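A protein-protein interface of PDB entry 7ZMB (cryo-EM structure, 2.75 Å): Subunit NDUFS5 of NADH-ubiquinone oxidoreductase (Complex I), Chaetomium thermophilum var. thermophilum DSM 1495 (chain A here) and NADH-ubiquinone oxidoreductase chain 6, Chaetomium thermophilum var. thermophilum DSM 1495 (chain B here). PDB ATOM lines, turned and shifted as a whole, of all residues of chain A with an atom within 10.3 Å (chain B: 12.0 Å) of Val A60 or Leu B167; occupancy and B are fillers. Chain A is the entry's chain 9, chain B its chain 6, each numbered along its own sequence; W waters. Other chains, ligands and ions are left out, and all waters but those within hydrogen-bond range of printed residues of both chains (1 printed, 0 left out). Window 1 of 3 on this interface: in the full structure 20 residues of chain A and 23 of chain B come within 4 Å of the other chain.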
ATOM      1  N   GLU A  49      35.748 -22.584 -18.143  1.00  0.00           N
ATOM      2  CA  GLU A  49      34.463 -22.624 -17.395  1.00  0.00           C
ATOM      3  C   GLU A  49      33.694 -21.321 -17.590  1.00  0.00           C
ATOM      4  O   GLU A  49      32.464 -21.388 -17.708  1.00  0.00           O
ATOM      5  CB  GLU A  49      34.654 -23.074 -15.946  1.00  0.00           C
ATOM      6  CG  GLU A  49      33.377 -23.158 -15.142  1.00  0.00           C
ATOM      7  CD  GLU A  49      32.265 -23.988 -15.756  1.00  0.00           C
ATOM      8  OE1 GLU A  49      32.571 -24.964 -16.445  1.00  0.00           O
ATOM      9  OE2 GLU A  49      31.094 -23.650 -15.537  1.00  0.00           O
ATOM     10  N   HIS A  52      32.445 -21.768 -21.549  1.00  0.00           N
ATOM     11  CA  HIS A  52      31.431 -22.770 -21.965  1.00  0.00           C
ATOM     12  C   HIS A  52      30.392 -23.081 -20.876  1.00  0.00           C
ATOM     13  O   HIS A  52      29.240 -23.354 -21.256  1.00  0.00           O
ATOM     14  CB  HIS A  52      32.197 -23.964 -22.530  1.00  0.00           C
ATOM     15  CG  HIS A  52      33.193 -23.534 -23.550  1.00  0.00           C
ATOM     16  ND1 HIS A  52      32.845 -22.742 -24.627  1.00  0.00           N
ATOM     17  CD2 HIS A  52      34.522 -23.741 -23.647  1.00  0.00           C
ATOM     18  CE1 HIS A  52      33.915 -22.496 -25.350  1.00  0.00           C
ATOM     19  NE2 HIS A  52      34.952 -23.102 -24.773  1.00  0.00           N
ATOM     20  N   HIS A  53      30.769 -23.051 -19.590  1.00  0.00           N
ATOM     21  CA  HIS A  53      29.823 -23.249 -18.454  1.00  0.00           C
ATOM     22  C   HIS A  53      29.438 -24.717 -18.202  1.00  0.00           C
ATOM     23  O   HIS A  53      28.408 -24.910 -17.550  1.00  0.00           O
ATOM     24  CB  HIS A  53      28.573 -22.364 -18.575  1.00  0.00           C
ATOM     25  CG  HIS A  53      28.839 -20.932 -18.880  1.00  0.00           C
ATOM     26  ND1 HIS A  53      29.359 -20.062 -17.948  1.00  0.00           N
ATOM     27  CD2 HIS A  53      28.633 -20.211 -20.002  1.00  0.00           C
ATOM     28  CE1 HIS A  53      29.477 -18.869 -18.487  1.00  0.00           C
ATOM     29  NE2 HIS A  53      29.038 -18.934 -19.743  1.00  0.00           N
ATOM     30  N   ARG A  54      30.224 -25.700 -18.649  1.00  0.00           N
ATOM     31  CA  ARG A  54      29.845 -27.135 -18.496  1.00  0.00           C
ATOM     32  C   ARG A  54      29.766 -27.556 -17.025  1.00  0.00           C
ATOM     33  O   ARG A  54      28.855 -28.327 -16.697  1.00  0.00           O
ATOM     34  CB  ARG A  54      30.796 -28.055 -19.257  1.00  0.00           C
ATOM     35  CG  ARG A  54      30.993 -27.661 -20.713  1.00  0.00           C
ATOM     36  CD  ARG A  54      31.619 -28.740 -21.571  1.00  0.00           C
ATOM     37  NE  ARG A  54      30.628 -29.665 -22.104  1.00  0.00           N
ATOM     38  CZ  ARG A  54      30.389 -30.879 -21.625  1.00  0.00           C
ATOM     39  NH1 ARG A  54      29.461 -31.638 -22.181  1.00  0.00           N
ATOM     40  NH2 ARG A  54      31.085 -31.336 -20.599  1.00  0.00           N
ATOM     41  N   LYS A  55      30.682 -27.075 -16.181  1.00  0.00           N
ATOM     42  CA  LYS A  55      30.719 -27.455 -14.747  1.00  0.00           C
ATOM     43  C   LYS A  55      29.573 -26.785 -13.979  1.00  0.00           C
ATOM     44  O   LYS A  55      29.060 -27.414 -13.050  1.00  0.00           O
ATOM     45  CB  LYS A  55      32.085 -27.086 -14.164  1.00  0.00           C
ATOM     46  CG  LYS A  55      33.293 -27.694 -14.860  1.00  0.00           C
ATOM     47  CD  LYS A  55      34.597 -27.237 -14.259  1.00  0.00           C
ATOM     48  CE  LYS A  55      34.744 -27.647 -12.811  1.00  0.00           C
ATOM     49  NZ  LYS A  55      35.929 -27.029 -12.174  1.00  0.00           N
ATOM     50  N   GLU A  56      29.196 -25.560 -14.347  1.00  0.00           N
ATOM     51  CA  GLU A  56      28.102 -24.805 -13.673  1.00  0.00           C
ATOM     52  C   GLU A  56      26.781 -25.298 -14.230  1.00  0.00           C
ATOM     53  O   GLU A  56      25.758 -25.160 -13.552  1.00  0.00           O
ATOM     54  CB  GLU A  56      28.305 -23.301 -13.819  1.00  0.00           C
ATOM     55  CG  GLU A  56      27.165 -22.440 -13.347  1.00  0.00           C
ATOM     56  CD  GLU A  56      27.262 -21.047 -13.939  1.00  0.00           C
ATOM     57  OE1 GLU A  56      28.092 -20.848 -14.840  1.00  0.00           O
ATOM     58  OE2 GLU A  56      26.516 -20.174 -13.492  1.00  0.00           O
ATOM     59  N   ALA A  57      26.853 -25.966 -15.368  1.00  0.00           N
ATOM     60  CA  ALA A  57      25.638 -26.523 -15.975  1.00  0.00           C
ATOM     61  C   ALA A  57      25.436 -27.837 -15.253  1.00  0.00           C
ATOM     62  O   ALA A  57      24.293 -28.222 -15.027  1.00  0.00           O
ATOM     63  CB  ALA A  57      25.856 -26.749 -17.445  1.00  0.00           C
ATOM     64  N   ALA A  58      26.543 -28.441 -14.843  1.00  0.00           N
ATOM     65  CA  ALA A  58      26.431 -29.776 -14.217  1.00  0.00           C
ATOM     66  C   ALA A  58      25.965 -29.634 -12.770  1.00  0.00           C
ATOM     67  O   ALA A  58      25.178 -30.469 -12.333  1.00  0.00           O
ATOM     68  CB  ALA A  58      27.739 -30.489 -14.339  1.00  0.00           C
ATOM     69  N   ARG A  59      26.441 -28.610 -12.065  1.00  0.00           N
ATOM     70  CA  ARG A  59      26.015 -28.358 -10.674  1.00  0.00           C
ATOM     71  C   ARG A  59      24.530 -28.026 -10.622  1.00  0.00           C
ATOM     72  O   ARG A  59      23.829 -28.619  -9.791  1.00  0.00           O
ATOM     73  CB  ARG A  59      26.789 -27.160 -10.131  1.00  0.00           C
ATOM     74  CG  ARG A  59      26.398 -26.738  -8.726  1.00  0.00           C
ATOM     75  CD  ARG A  59      27.081 -25.438  -8.356  1.00  0.00           C
ATOM     76  NE  ARG A  59      26.429 -24.798  -7.228  1.00  0.00           N
ATOM     77  CZ  ARG A  59      25.346 -24.039  -7.324  1.00  0.00           C
ATOM     78  NH1 ARG A  59      24.788 -23.823  -8.502  1.00  0.00           N
ATOM     79  NH2 ARG A  59      24.827 -23.497  -6.238  1.00  0.00           N
ATOM     80  N   VAL A  60      24.064 -27.154 -11.510  1.00  0.00           N
ATOM     81  CA  VAL A  60      22.645 -26.717 -11.451  1.00  0.00           C
ATOM     82  C   VAL A  60      21.758 -27.906 -11.807  1.00  0.00           C
ATOM     83  O   VAL A  60      20.696 -28.010 -11.213  1.00  0.00           O
ATOM     84  CB  VAL A  60      22.384 -25.466 -12.312  1.00  0.00           C
ATOM     85  CG1 VAL A  60      20.909 -25.121 -12.412  1.00  0.00           C
ATOM     86  CG2 VAL A  60      23.170 -24.275 -11.787  1.00  0.00           C
ATOM     87  N   ARG A  61      22.220 -28.818 -12.659  1.00  0.00           N
ATOM     88  CA  ARG A  61      21.394 -29.984 -12.966  1.00  0.00           C
ATOM     89  C   ARG A  61      21.207 -30.862 -11.738  1.00  0.00           C
ATOM     90  O   ARG A  61      20.096 -31.320 -11.454  1.00  0.00           O
ATOM     91  CB  ARG A  61      22.016 -30.792 -14.104  1.00  0.00           C
ATOM     92  CG  ARG A  61      22.012 -30.083 -15.418  1.00  0.00           C
ATOM     93  CD  ARG A  61      22.608 -30.922 -16.525  1.00  0.00           C
ATOM     94  NE  ARG A  61      22.677 -30.174 -17.773  1.00  0.00           N
ATOM     95  CZ  ARG A  61      21.701 -30.128 -18.672  1.00  0.00           C
ATOM     96  NH1 ARG A  61      20.576 -30.797 -18.464  1.00  0.00           N
ATOM     97  NH2 ARG A  61      21.852 -29.417 -19.781  1.00  0.00           N
ATOM     98  N   ALA A  62      22.290 -31.113 -11.006  1.00  0.00           N
ATOM     99  CA  ALA A  62      22.204 -31.913  -9.790  1.00  0.00           C
ATOM    100  C   ALA A  62      21.297 -31.258  -8.757  1.00  0.00           C
ATOM    101  O   ALA A  62      20.375 -31.891  -8.231  1.00  0.00           O
ATOM    102  CB  ALA A  62      23.602 -32.127  -9.215  1.00  0.00           C
ATOM    103  N   LEU A  63      21.538 -29.982  -8.455  1.00  0.00           N
ATOM    104  CA  LEU A  63      20.808 -29.345  -7.370  1.00  0.00           C
ATOM    105  C   LEU A  63      19.350 -29.134  -7.752  1.00  0.00           C
ATOM    106  O   LEU A  63      18.461 -29.241  -6.902  1.00  0.00           O
ATOM    107  CB  LEU A  63      21.464 -28.015  -7.012  1.00  0.00           C
ATOM    108  CG  LEU A  63      21.020 -27.223  -5.772  1.00  0.00           C
ATOM    109  CD1 LEU A  63      22.187 -26.371  -5.323  1.00  0.00           C
ATOM    110  CD2 LEU A  63      19.751 -26.386  -5.898  1.00  0.00           C
ATOM    111  N   GLN A  64      19.090 -28.846  -9.026  1.00  0.00           N
ATOM    112  CA  GLN A  64      17.729 -28.620  -9.487  1.00  0.00           C
ATOM    113  C   GLN A  64      16.884 -29.884  -9.396  1.00  0.00           C
ATOM    114  O   GLN A  64      15.687 -29.806  -9.104  1.00  0.00           O
ATOM    115  CB  GLN A  64      17.760 -28.108 -10.921  1.00  0.00           C
ATOM    116  CG  GLN A  64      16.432 -27.743 -11.507  1.00  0.00           C
ATOM    117  CD  GLN A  64      16.589 -27.207 -12.894  1.00  0.00           C
ATOM    118  OE1 GLN A  64      17.694 -27.149 -13.423  1.00  0.00           O
ATOM    119  NE2 GLN A  64      15.496 -26.813 -13.498  1.00  0.00           N
ATOM    120  N   ALA A  65      17.470 -31.045  -9.667  1.00  0.00           N
ATOM    121  CA  ALA A  65      16.726 -32.286  -9.491  1.00  0.00           C
ATOM    122  C   ALA A  65      16.519 -32.577  -8.012  1.00  0.00           C
ATOM    123  O   ALA A  65      15.421 -32.956  -7.590  1.00  0.00           O
ATOM    124  CB  ALA A  65      17.454 -33.438 -10.179  1.00  0.00           C
ATOM    125  N   ALA A  66      17.560 -32.371  -7.208  1.00  0.00           N
ATOM    126  CA  ALA A  66      17.438 -32.490  -5.762  1.00  0.00           C
ATOM    127  C   ALA A  66      16.415 -31.509  -5.204  1.00  0.00           C
ATOM    128  O   ALA A  66      15.670 -31.830  -4.276  1.00  0.00           O
ATOM    129  CB  ALA A  66      18.804 -32.264  -5.112  1.00  0.00           C
ATOM    130  N   TYR A  67      16.395 -30.285  -5.733  1.00  0.00           N
ATOM    131  CA  TYR A  67      15.509 -29.269  -5.182  1.00  0.00           C
ATOM    132  C   TYR A  67      14.056 -29.584  -5.493  1.00  0.00           C
ATOM    133  O   TYR A  67      13.200 -29.553  -4.603  1.00  0.00           O
ATOM    134  CB  TYR A  67      15.898 -27.885  -5.705  1.00  0.00           C
ATOM    135  CG  TYR A  67      14.949 -26.772  -5.315  1.00  0.00           C
ATOM    136  CD1 TYR A  67      13.782 -26.539  -6.031  1.00  0.00           C
ATOM    137  CD2 TYR A  67      15.246 -25.925  -4.262  1.00  0.00           C
ATOM    138  CE1 TYR A  67      12.933 -25.524  -5.687  1.00  0.00           C
ATOM    139  CE2 TYR A  67      14.399 -24.910  -3.906  1.00  0.00           C
ATOM    140  CZ  TYR A  67      13.245 -24.710  -4.622  1.00  0.00           C
ATOM    141  OH  TYR A  67      12.395 -23.689  -4.273  1.00  0.00           O
ATOM    142  N   ARG A  68      13.759 -29.892  -6.752  1.00  0.00           N
ATOM    143  CA  ARG A  68      12.381 -30.164  -7.125  1.00  0.00           C
ATOM    144  C   ARG A  68      11.843 -31.409  -6.435  1.00  0.00           C
ATOM    145  O   ARG A  68      10.695 -31.417  -5.979  1.00  0.00           O
ATOM    146  CB  ARG A  68      12.255 -30.271  -8.640  1.00  0.00           C
ATOM    147  CG  ARG A  68      12.484 -28.960  -9.356  1.00  0.00           C
ATOM    148  CD  ARG A  68      12.345 -29.134 -10.836  1.00  0.00           C
ATOM    149  NE  ARG A  68      12.568 -27.893 -11.559  1.00  0.00           N
ATOM    150  CZ  ARG A  68      12.553 -27.802 -12.879  1.00  0.00           C
ATOM    151  NH1 ARG A  68      12.738 -26.630 -13.468  1.00  0.00           N
ATOM    152  NH2 ARG A  68      12.344 -28.884 -13.614  1.00  0.00           N
ATOM    153  N   LEU B   7      11.905 -19.920  -3.116  1.00  0.00           N
ATOM    154  CA  LEU B   7      12.221 -19.671  -4.554  1.00  0.00           C
ATOM    155  C   LEU B   7      10.939 -19.340  -5.299  1.00  0.00           C
ATOM    156  O   LEU B   7      10.032 -20.189  -5.297  1.00  0.00           O
ATOM    157  CB  LEU B   7      12.954 -20.845  -5.218  1.00  0.00           C
ATOM    158  CG  LEU B   7      14.486 -20.830  -5.162  1.00  0.00           C
ATOM    159  CD1 LEU B   7      15.058 -21.969  -5.992  1.00  0.00           C
ATOM    160  CD2 LEU B   7      15.049 -19.505  -5.643  1.00  0.00           C
ATOM    161  N   LEU B   9       8.995 -18.449  -8.788  1.00  0.00           N
ATOM    162  CA  LEU B   9       9.005 -18.335 -10.259  1.00  0.00           C
ATOM    163  C   LEU B   9       7.778 -17.494 -10.589  1.00  0.00           C
ATOM    164  O   LEU B   9       6.681 -17.866 -10.201  1.00  0.00           O
ATOM    165  CB  LEU B   9       8.977 -19.727 -10.893  1.00  0.00           C
ATOM    166  CG  LEU B   9       9.713 -19.880 -12.222  1.00  0.00           C
ATOM    167  CD1 LEU B   9       9.765 -21.341 -12.635  1.00  0.00           C
ATOM    168  CD2 LEU B   9       9.058 -19.051 -13.315  1.00  0.00           C
ATOM    169  N   HIS B  20      11.100 -17.932 -27.630  1.00  0.00           N
ATOM    170  CA  HIS B  20      12.215 -18.648 -28.303  1.00  0.00           C
ATOM    171  C   HIS B  20      11.632 -19.652 -29.294  1.00  0.00           C
ATOM    172  O   HIS B  20      12.424 -20.308 -29.997  1.00  0.00           O
ATOM    173  CB  HIS B  20      13.171 -19.263 -27.279  1.00  0.00           C
ATOM    174  CG  HIS B  20      12.591 -20.428 -26.549  1.00  0.00           C
ATOM    175  ND1 HIS B  20      11.857 -20.280 -25.392  1.00  0.00           N
ATOM    176  CD2 HIS B  20      12.628 -21.753 -26.809  1.00  0.00           C
ATOM    177  CE1 HIS B  20      11.466 -21.464 -24.967  1.00  0.00           C
ATOM    178  NE2 HIS B  20      11.928 -22.384 -25.819  1.00  0.00           N
ATOM    179  N   TYR B 127      29.793 -26.011 -25.828  1.00  0.00           N
ATOM    180  CA  TYR B 127      28.571 -26.076 -24.979  1.00  0.00           C
ATOM    181  C   TYR B 127      27.678 -24.847 -25.170  1.00  0.00           C
ATOM    182  O   TYR B 127      26.452 -25.022 -25.238  1.00  0.00           O
ATOM    183  CB  TYR B 127      28.954 -26.309 -23.521  1.00  0.00           C
ATOM    184  CG  TYR B 127      27.888 -26.952 -22.675  1.00  0.00           C
ATOM    185  CD1 TYR B 127      27.451 -28.238 -22.937  1.00  0.00           C
ATOM    186  CD2 TYR B 127      27.333 -26.282 -21.601  1.00  0.00           C
ATOM    187  CE1 TYR B 127      26.478 -28.844 -22.161  1.00  0.00           C
ATOM    188  CE2 TYR B 127      26.358 -26.872 -20.816  1.00  0.00           C
ATOM    189  CZ  TYR B 127      25.929 -28.157 -21.094  1.00  0.00           C
ATOM    190  OH  TYR B 127      24.967 -28.743 -20.324  1.00  0.00           O
ATOM    191  N   GLY B 128      28.271 -23.658 -25.292  1.00  0.00           N
ATOM    192  CA  GLY B 128      27.480 -22.442 -25.560  1.00  0.00           C
ATOM    193  C   GLY B 128      26.452 -22.610 -26.661  1.00  0.00           C
ATOM    194  O   GLY B 128      25.353 -22.049 -26.517  1.00  0.00           O
ATOM    195  N   VAL B 129      26.751 -23.398 -27.691  1.00  0.00           N
ATOM    196  CA  VAL B 129      25.850 -23.468 -28.831  1.00  0.00           C
ATOM    197  C   VAL B 129      24.978 -24.715 -28.791  1.00  0.00           C
ATOM    198  O   VAL B 129      23.785 -24.644 -29.082  1.00  0.00           O
ATOM    199  CB  VAL B 129      26.659 -23.393 -30.143  1.00  0.00           C
ATOM    200  CG1 VAL B 129      25.726 -23.207 -31.331  1.00  0.00           C
ATOM    201  CG2 VAL B 129      27.686 -22.266 -30.067  1.00  0.00           C
ATOM    202  N   ILE B 130      25.548 -25.866 -28.421  1.00  0.00           N
ATOM    203  CA  ILE B 130      24.792 -27.116 -28.427  1.00  0.00           C
ATOM    204  C   ILE B 130      23.681 -27.150 -27.390  1.00  0.00           C
ATOM    205  O   ILE B 130      22.889 -28.098 -27.382  1.00  0.00           O
ATOM    206  CB  ILE B 130      25.726 -28.321 -28.210  1.00  0.00           C
ATOM    207  CG1 ILE B 130      26.732 -28.015 -27.102  1.00  0.00           C
ATOM    208  CG2 ILE B 130      26.436 -28.676 -29.500  1.00  0.00           C
ATOM    209  CD1 ILE B 130      27.658 -29.164 -26.775  1.00  0.00           C
ATOM    210  N   ILE B 131      23.609 -26.150 -26.510  1.00  0.00           N
ATOM    211  CA  ILE B 131      22.478 -26.038 -25.600  1.00  0.00           C
ATOM    212  C   ILE B 131      21.186 -25.878 -26.399  1.00  0.00           C
ATOM    213  O   ILE B 131      21.159 -25.252 -27.466  1.00  0.00           O
ATOM    214  CB  ILE B 131      22.691 -24.862 -24.631  1.00  0.00           C
ATOM    215  CG1 ILE B 131      23.733 -25.237 -23.583  1.00  0.00           C
ATOM    216  CG2 ILE B 131      21.394 -24.447 -23.954  1.00  0.00           C
ATOM    217  CD1 ILE B 131      23.303 -26.377 -22.712  1.00  0.00           C
ATOM    218  N   SER B 132      20.104 -26.465 -25.879  1.00  0.00           N
ATOM    219  CA  SER B 132      18.784 -26.423 -26.508  1.00  0.00           C
ATOM    220  C   SER B 132      18.824 -27.049 -27.903  1.00  0.00           C
ATOM    221  O   SER B 132      18.573 -26.401 -28.921  1.00  0.00           O
ATOM    222  CB  SER B 132      18.241 -24.988 -26.555  1.00  0.00           C
ATOM    223  OG  SER B 132      18.923 -24.211 -27.524  1.00  0.00           O
ATOM    224  N   ASN B 133      19.155 -28.336 -27.926  1.00  0.00           N
ATOM    225  CA  ASN B 133      19.224 -29.092 -29.170  1.00  0.00           C
ATOM    226  C   ASN B 133      17.829 -29.409 -29.699  1.00  0.00           C
ATOM    227  O   ASN B 133      17.505 -30.564 -29.975  1.00  0.00           O
ATOM    228  CB  ASN B 133      20.016 -30.386 -28.965  1.00  0.00           C
ATOM    229  N   LYS B 164      13.182 -33.954 -18.797  1.00  0.00           N
ATOM    230  CA  LYS B 164      12.184 -33.007 -18.313  1.00  0.00           C
ATOM    231  C   LYS B 164      12.783 -32.057 -17.281  1.00  0.00           C
ATOM    232  O   LYS B 164      12.060 -31.341 -16.591  1.00  0.00           O
ATOM    233  CB  LYS B 164      10.988 -33.749 -17.713  1.00  0.00           C
ATOM    234  N   ASN B 165      14.109 -32.060 -17.180  1.00  0.00           N
ATOM    235  CA  ASN B 165      14.841 -31.190 -16.264  1.00  0.00           C
ATOM    236  C   ASN B 165      15.726 -30.274 -17.102  1.00  0.00           C
ATOM    237  O   ASN B 165      16.893 -30.586 -17.357  1.00  0.00           O
ATOM    238  CB  ASN B 165      15.665 -31.994 -15.257  1.00  0.00           C
ATOM    239  N   ASP B 166      15.170 -29.148 -17.528  1.00  0.00           N
ATOM    240  CA  ASP B 166      15.886 -28.185 -18.349  1.00  0.00           C
ATOM    241  C   ASP B 166      16.598 -27.162 -17.476  1.00  0.00           C
ATOM    242  O   ASP B 166      16.285 -26.987 -16.299  1.00  0.00           O
ATOM    243  CB  ASP B 166      14.930 -27.473 -19.312  1.00  0.00           C
ATOM    244  CG  ASP B 166      14.315 -28.415 -20.325  1.00  0.00           C
ATOM    245  OD1 ASP B 166      14.850 -29.528 -20.507  1.00  0.00           O
ATOM    246  OD2 ASP B 166      13.298 -28.040 -20.944  1.00  0.00           O
ATOM    247  N   LEU B 167      17.575 -26.490 -18.070  1.00  0.00           N
ATOM    248  CA  LEU B 167      18.272 -25.408 -17.398  1.00  0.00           C
ATOM    249  C   LEU B 167      17.661 -24.085 -17.805  1.00  0.00           C
ATOM    250  O   LEU B 167      17.020 -23.971 -18.850  1.00  0.00           O
ATOM    251  CB  LEU B 167      19.766 -25.412 -17.719  1.00  0.00           C
ATOM    252  CG  LEU B 167      20.547 -26.533 -17.051  1.00  0.00           C
ATOM    253  CD1 LEU B 167      22.031 -26.336 -17.233  1.00  0.00           C
ATOM    254  CD2 LEU B 167      20.185 -26.627 -15.585  1.00  0.00           C
ATOM    255  N   PHE B 168      17.847 -23.094 -16.945  1.00  0.00           N
ATOM    256  CA  PHE B 168      17.327 -21.740 -17.245  1.00  0.00           C
ATOM    257  C   PHE B 168      18.469 -20.751 -17.035  1.00  0.00           C
ATOM    258  O   PHE B 168      19.097 -20.761 -15.960  1.00  0.00           O
ATOM    259  CB  PHE B 168      16.085 -21.431 -16.411  1.00  0.00           C
ATOM    260  CG  PHE B 168      14.883 -22.281 -16.743  1.00  0.00           C
ATOM    261  CD1 PHE B 168      14.041 -21.944 -17.790  1.00  0.00           C
ATOM    262  CD2 PHE B 168      14.594 -23.421 -16.011  1.00  0.00           C
ATOM    263  CE1 PHE B 168      12.939 -22.725 -18.098  1.00  0.00           C
ATOM    264  CE2 PHE B 168      13.492 -24.202 -16.318  1.00  0.00           C
ATOM    265  CZ  PHE B 168      12.667 -23.852 -17.360  1.00  0.00           C
ATOM    266  N   PHE B 169      18.765 -19.972 -18.073  1.00  0.00           N
ATOM    267  CA  PHE B 169      19.807 -18.930 -17.944  1.00  0.00           C
ATOM    268  C   PHE B 169      19.258 -17.828 -17.044  1.00  0.00           C
ATOM    269  O   PHE B 169      18.082 -17.474 -17.181  1.00  0.00           O
ATOM    270  CB  PHE B 169      20.244 -18.439 -19.326  1.00  0.00           C
ATOM    271  CG  PHE B 169      20.821 -19.482 -20.247  1.00  0.00           C
ATOM    272  CD1 PHE B 169      22.172 -19.778 -20.226  1.00  0.00           C
ATOM    273  CD2 PHE B 169      20.015 -20.151 -21.153  1.00  0.00           C
ATOM    274  CE1 PHE B 169      22.706 -20.723 -21.088  1.00  0.00           C
ATOM    275  CE2 PHE B 169      20.549 -21.103 -22.007  1.00  0.00           C
ATOM    276  CZ  PHE B 169      21.892 -21.388 -21.972  1.00  0.00           C
ATOM    277  N   ILE B 170      20.089 -17.328 -16.133  1.00  0.00           N
ATOM    278  CA  ILE B 170      19.648 -16.266 -15.188  1.00  0.00           C
ATOM    279  C   ILE B 170      20.444 -14.992 -15.478  1.00  0.00           C
ATOM    280  O   ILE B 170      21.667 -15.081 -15.649  1.00  0.00           O
ATOM    281  CB  ILE B 170      19.759 -16.752 -13.730  1.00  0.00           C
ATOM    282  CG1 ILE B 170      19.048 -15.814 -12.754  1.00  0.00           C
ATOM    283  CG2 ILE B 170      21.192 -17.045 -13.319  1.00  0.00           C
ATOM    284  CD1 ILE B 170      17.558 -16.009 -12.714  1.00  0.00           C
ATOM    285  N   THR B 171      19.753 -13.858 -15.589  1.00  0.00           N
ATOM    286  CA  THR B 171      20.443 -12.564 -15.836  1.00  0.00           C
ATOM    287  C   THR B 171      20.048 -11.539 -14.768  1.00  0.00           C
ATOM    288  O   THR B 171      18.930 -11.621 -14.261  1.00  0.00           O
ATOM    289  CB  THR B 171      20.211 -12.053 -17.262  1.00  0.00           C
ATOM    290  OG1 THR B 171      18.857 -11.623 -17.398  1.00  0.00           O
ATOM    291  CG2 THR B 171      20.546 -13.077 -18.321  1.00  0.00           C
HETATM  292  O   HOH W   1      17.061 -24.215 -14.142  1.00  0.00           O
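Val A60 touches just one residue of chain B: Leu B167.
Of the printed residues of chain A, Leu B167 touches Ala A57, Val A60, Arg A61 and Gln A64.
Of chain B, only Tyr B127 (3.4 Å) and Leu B167 (3.7 Å) come within 4 Å of Ala A57.
No residue of chain B comes within 4 Å of Arg A59.
No residue of chain B comes within 4 Å of Ala A62.
Leu A63 touches none of the printed residues of chain B.
Of chain A, only Gln A64 (2.9 Å) comes within 4 Å of Asp B166.
Of the printed residues of chain A, Phe B168 touches Arg A68 (3.8 Å).
Of the printed residues of chain B, Arg A54 touches Tyr B127.
Of the printed residues of chain A, Leu B7 touches Tyr A67.
Of the printed residues of chain A, Tyr B127 touches His A52, Arg A54, Ala A57 and Arg A61.
Asn B133 touches none of the printed residues of chain A.
Ile B131 touches none of the printed residues of chain A.
His A52 touches Tyr B127 (O to CD2, 3.5 Å).
Arg A54 touches Tyr B127 (NE to CD1, 3.6 Å).
CB of Ala A57 touches CE2 of Tyr B127, at 3.4 Å.
CD1 of Leu B167 touches O of Ala A57, 3.7 Å away.
CG1 of Val A60 touches CD2 of Leu B167, 3.6 Å away.
NH1 of Arg A61 touches O of Asn B165, 3.9 Å away.
Leu B167 touches Arg A61.
CB of Leu B7 touches OH of Tyr A67, at 3.0 Å.
NH2 of Arg A68 touches O of Lys B164 (3.9 Å).
Arg A68 touches Phe B168 (NH1 to CE2, 3.8 Å).
The side-chain carboxylate (OE1) of Glu A49 is in hydrogen-bond range of the backbone NH (N) of Arg A54, 3.3 Å away.
NE2 of Gln A64 sits close to NH1 of Arg A68.
Water W1 lies within hydrogen-bond range of OE1 of Gln A64 (3.1 Å) and N of Phe B168 (3.1 Å).
OH of Tyr B127 is in hydrogen-bond range of NH2 of Arg A61, at 3.2 Å.
The backbone carbonyl oxygen of Asp B166 lies within hydrogen-bond range of the side-chain amide nitrogen of Gln A64.
Of the 18 printed residues of chain A, 8 touch a printed residue of chain B.
Hydrophobic or aromatic side chains of chain A within 4 Å of the printed part of chain B: Ala A57, Val A60 and Tyr A67.
Among the printed residues, 13 pairs touch across the chains.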
